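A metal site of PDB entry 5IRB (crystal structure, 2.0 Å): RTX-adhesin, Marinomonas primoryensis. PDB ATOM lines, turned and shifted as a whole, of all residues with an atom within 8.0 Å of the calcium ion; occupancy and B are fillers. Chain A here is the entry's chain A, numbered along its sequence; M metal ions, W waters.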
ATOM      1  N   ILE A 119      22.151   5.419 -20.634  1.00  0.00           N
ATOM      2  CA  ILE A 119      20.692   5.253 -20.622  1.00  0.00           C
ATOM      3  C   ILE A 119      20.013   6.457 -19.971  1.00  0.00           C
ATOM      4  O   ILE A 119      19.971   6.551 -18.753  1.00  0.00           O
ATOM      5  CB  ILE A 119      20.291   3.940 -19.910  1.00  0.00           C
ATOM      6  CG1 ILE A 119      21.038   2.734 -20.495  1.00  0.00           C
ATOM      7  CG2 ILE A 119      18.775   3.706 -19.971  1.00  0.00           C
ATOM      8  CD1 ILE A 119      20.918   2.553 -22.038  1.00  0.00           C
ATOM      9  N   THR A 120      19.576   7.408 -20.784  1.00  0.00           N
ATOM     10  CA  THR A 120      19.171   8.749 -20.382  1.00  0.00           C
ATOM     11  C   THR A 120      20.386   9.494 -19.866  1.00  0.00           C
ATOM     12  O   THR A 120      21.481   8.940 -19.771  1.00  0.00           O
ATOM     13  CB  THR A 120      18.034   8.795 -19.290  1.00  0.00           C
ATOM     14  OG1 THR A 120      18.625   8.572 -18.006  1.00  0.00           O
ATOM     15  CG2 THR A 120      16.948   7.755 -19.538  1.00  0.00           C
ATOM     16  N   SER A 121      20.186  10.778 -19.544  1.00  0.00           N
ATOM     17  CA  SER A 121      21.275  11.692 -19.232  1.00  0.00           C
ATOM     18  C   SER A 121      22.230  11.263 -18.129  1.00  0.00           C
ATOM     19  O   SER A 121      23.422  11.518 -18.211  1.00  0.00           O
ATOM     20  CB  SER A 121      20.674  13.033 -18.804  1.00  0.00           C
ATOM     21  OG  SER A 121      21.121  14.073 -19.657  1.00  0.00           O
ATOM     22  N   ASP A 122      21.714  10.605 -17.089  1.00  0.00           N
ATOM     23  CA  ASP A 122      22.522  10.276 -15.918  1.00  0.00           C
ATOM     24  C   ASP A 122      22.741   8.782 -15.776  1.00  0.00           C
ATOM     25  O   ASP A 122      23.246   8.354 -14.743  1.00  0.00           O
ATOM     26  CB  ASP A 122      21.866  10.778 -14.624  1.00  0.00           C
ATOM     27  CG  ASP A 122      20.454  10.205 -14.424  1.00  0.00           C
ATOM     28  OD1 ASP A 122      19.969   9.464 -15.301  1.00  0.00           O
ATOM     29  OD2 ASP A 122      19.829  10.507 -13.389  1.00  0.00           O
ATOM     30  N   ASP A 123      22.313   8.004 -16.778  1.00  0.00           N
ATOM     31  CA  ASP A 123      22.503   6.558 -16.764  1.00  0.00           C
ATOM     32  C   ASP A 123      21.657   5.929 -15.639  1.00  0.00           C
ATOM     33  O   ASP A 123      21.941   4.835 -15.156  1.00  0.00           O
ATOM     34  CB  ASP A 123      23.980   6.180 -16.613  1.00  0.00           C
ATOM     35  CG  ASP A 123      24.328   4.876 -17.304  1.00  0.00           C
ATOM     36  OD1 ASP A 123      23.701   4.512 -18.334  1.00  0.00           O
ATOM     37  OD2 ASP A 123      25.217   4.195 -16.765  1.00  0.00           O
ATOM     38  N   VAL A 124      20.620   6.669 -15.228  1.00  0.00           N
ATOM     39  CA  VAL A 124      19.625   6.170 -14.277  1.00  0.00           C
ATOM     40  C   VAL A 124      18.203   6.275 -14.851  1.00  0.00           C
ATOM     41  O   VAL A 124      17.764   7.335 -15.330  1.00  0.00           O
ATOM     42  CB  VAL A 124      19.716   6.948 -12.929  1.00  0.00           C
ATOM     43  CG1 VAL A 124      18.662   6.465 -11.956  1.00  0.00           C
ATOM     44  CG2 VAL A 124      21.106   6.794 -12.350  1.00  0.00           C
ATOM     45  N   VAL A 125      17.455   5.179 -14.779  1.00  0.00           N
ATOM     46  CA  VAL A 125      16.069   5.202 -15.230  1.00  0.00           C
ATOM     47  C   VAL A 125      15.164   5.561 -14.058  1.00  0.00           C
ATOM     48  O   VAL A 125      14.979   4.756 -13.145  1.00  0.00           O
ATOM     49  CB  VAL A 125      15.622   3.867 -15.821  1.00  0.00           C
ATOM     50  CG1 VAL A 125      14.141   3.937 -16.186  1.00  0.00           C
ATOM     51  CG2 VAL A 125      16.441   3.540 -17.095  1.00  0.00           C
ATOM     52  N   ASN A 126      14.615   6.773 -14.075  1.00  0.00           N
ATOM     53  CA  ASN A 126      13.708   7.160 -12.993  1.00  0.00           C
ATOM     54  C   ASN A 126      12.253   6.782 -13.274  1.00  0.00           C
ATOM     55  O   ASN A 126      11.962   6.199 -14.318  1.00  0.00           O
ATOM     56  CB  ASN A 126      13.829   8.664 -12.658  1.00  0.00           C
ATOM     57  CG  ASN A 126      13.227   9.577 -13.733  1.00  0.00           C
ATOM     58  OD1 ASN A 126      12.472   9.129 -14.608  1.00  0.00           O
ATOM     59  ND2 ASN A 126      13.543  10.857 -13.641  1.00  0.00           N
ATOM     60  N   ALA A 127      11.360   7.136 -12.343  1.00  0.00           N
ATOM     61  CA  ALA A 127       9.946   6.764 -12.442  1.00  0.00           C
ATOM     62  C   ALA A 127       9.295   7.206 -13.741  1.00  0.00           C
ATOM     63  O   ALA A 127       8.670   6.420 -14.451  1.00  0.00           O
ATOM     64  CB  ALA A 127       9.157   7.333 -11.232  1.00  0.00           C
ATOM     65  N   GLU A 129      10.786   8.181 -16.531  1.00  0.00           N
ATOM     66  CA  GLU A 129      11.449   7.642 -17.702  1.00  0.00           C
ATOM     67  C   GLU A 129      10.979   6.216 -17.924  1.00  0.00           C
ATOM     68  O   GLU A 129      10.883   5.745 -19.062  1.00  0.00           O
ATOM     69  CB  GLU A 129      12.976   7.719 -17.521  1.00  0.00           C
ATOM     70  CG  GLU A 129      13.561   9.153 -17.587  1.00  0.00           C
ATOM     71  CD  GLU A 129      14.970   9.275 -16.969  1.00  0.00           C
ATOM     72  OE1 GLU A 129      15.297   8.438 -16.099  1.00  0.00           O
ATOM     73  OE2 GLU A 129      15.751  10.194 -17.373  1.00  0.00           O
ATOM     74  N   ILE A 134      12.534   5.577 -24.177  1.00  0.00           N
ATOM     75  CA  ILE A 134      13.895   6.031 -23.948  1.00  0.00           C
ATOM     76  C   ILE A 134      14.803   5.641 -25.141  1.00  0.00           C
ATOM     77  O   ILE A 134      14.789   4.506 -25.583  1.00  0.00           O
ATOM     78  CB  ILE A 134      14.470   5.437 -22.668  1.00  0.00           C
ATOM     79  CG1 ILE A 134      13.700   5.927 -21.434  1.00  0.00           C
ATOM     80  CG2 ILE A 134      15.937   5.773 -22.510  1.00  0.00           C
ATOM     81  CD1 ILE A 134      14.004   5.087 -20.213  1.00  0.00           C
ATOM     82  N   THR A 207      21.361   1.894 -13.901  1.00  0.00           N
ATOM     83  CA  THR A 207      20.671   1.610 -12.643  1.00  0.00           C
ATOM     84  C   THR A 207      19.232   2.095 -12.737  1.00  0.00           C
ATOM     85  O   THR A 207      18.900   2.954 -13.558  1.00  0.00           O
ATOM     86  CB  THR A 207      21.380   2.238 -11.432  1.00  0.00           C
ATOM     87  OG1 THR A 207      21.390   3.662 -11.522  1.00  0.00           O
ATOM     88  CG2 THR A 207      22.818   1.717 -11.372  1.00  0.00           C
ATOM     89  N   ASP A 209      16.051   3.630 -10.535  1.00  0.00           N
ATOM     90  CA  ASP A 209      15.636   4.317  -9.306  1.00  0.00           C
ATOM     91  C   ASP A 209      14.306   5.005  -9.563  1.00  0.00           C
ATOM     92  O   ASP A 209      14.270   6.092 -10.151  1.00  0.00           O
ATOM     93  CB  ASP A 209      16.666   5.349  -8.861  1.00  0.00           C
ATOM     94  CG  ASP A 209      16.351   5.937  -7.478  1.00  0.00           C
ATOM     95  OD1 ASP A 209      15.183   5.812  -7.032  1.00  0.00           O
ATOM     96  OD2 ASP A 209      17.264   6.545  -6.853  1.00  0.00           O
ATOM     97  N   ALA A 297      18.447  12.462  -6.405  1.00  0.00           N
ATOM     98  CA  ALA A 297      19.337  12.857  -7.503  1.00  0.00           C
ATOM     99  C   ALA A 297      18.831  12.357  -8.848  1.00  0.00           C
ATOM    100  O   ALA A 297      19.065  13.002  -9.867  1.00  0.00           O
ATOM    101  CB  ALA A 297      20.784  12.344  -7.267  1.00  0.00           C
ATOM    102  N   ALA A 298      18.128  11.221  -8.856  1.00  0.00           N
ATOM    103  CA  ALA A 298      17.509  10.726 -10.092  1.00  0.00           C
ATOM    104  C   ALA A 298      16.389  11.593 -10.616  1.00  0.00           C
ATOM    105  O   ALA A 298      15.995  11.445 -11.769  1.00  0.00           O
ATOM    106  CB  ALA A 298      16.991   9.316  -9.899  1.00  0.00           C
ATOM    107  N   GLY A 299      15.862  12.497  -9.783  1.00  0.00           N
ATOM    108  CA  GLY A 299      14.807  13.393 -10.221  1.00  0.00           C
ATOM    109  C   GLY A 299      13.408  12.973  -9.838  1.00  0.00           C
ATOM    110  O   GLY A 299      12.436  13.625 -10.235  1.00  0.00           O
HETATM  111 CA    CA M   1      17.654   9.399 -15.951  1.00  0.00          CA
HETATM  112  O   HOH W   1      17.302  10.243 -13.588  1.00  0.00           O
HETATM  113  O   HOH W   2      17.865  11.218 -16.705  1.00  0.00           O
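Four residues have an atom within 4 Å of the calcium ion: Thr 120, Asp 122, Val 124 and Glu 129.
Water W1 bridges the backbone carbonyl oxygen (O) of Ala 298 and the side-chain carboxylate (OD2) of Asp 122.
OD1 of Asn 126 is in hydrogen-bond range of N of Glu 129, 2.7 Å away.
The calcium ion is bound by water W2, O of Val 124, OD1 of Asp 122, OG1 of Thr 120, OE2 of Glu 129, water W1 and OE1 of Glu 129.
The calcium ion has seven donor atoms within binding distance.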
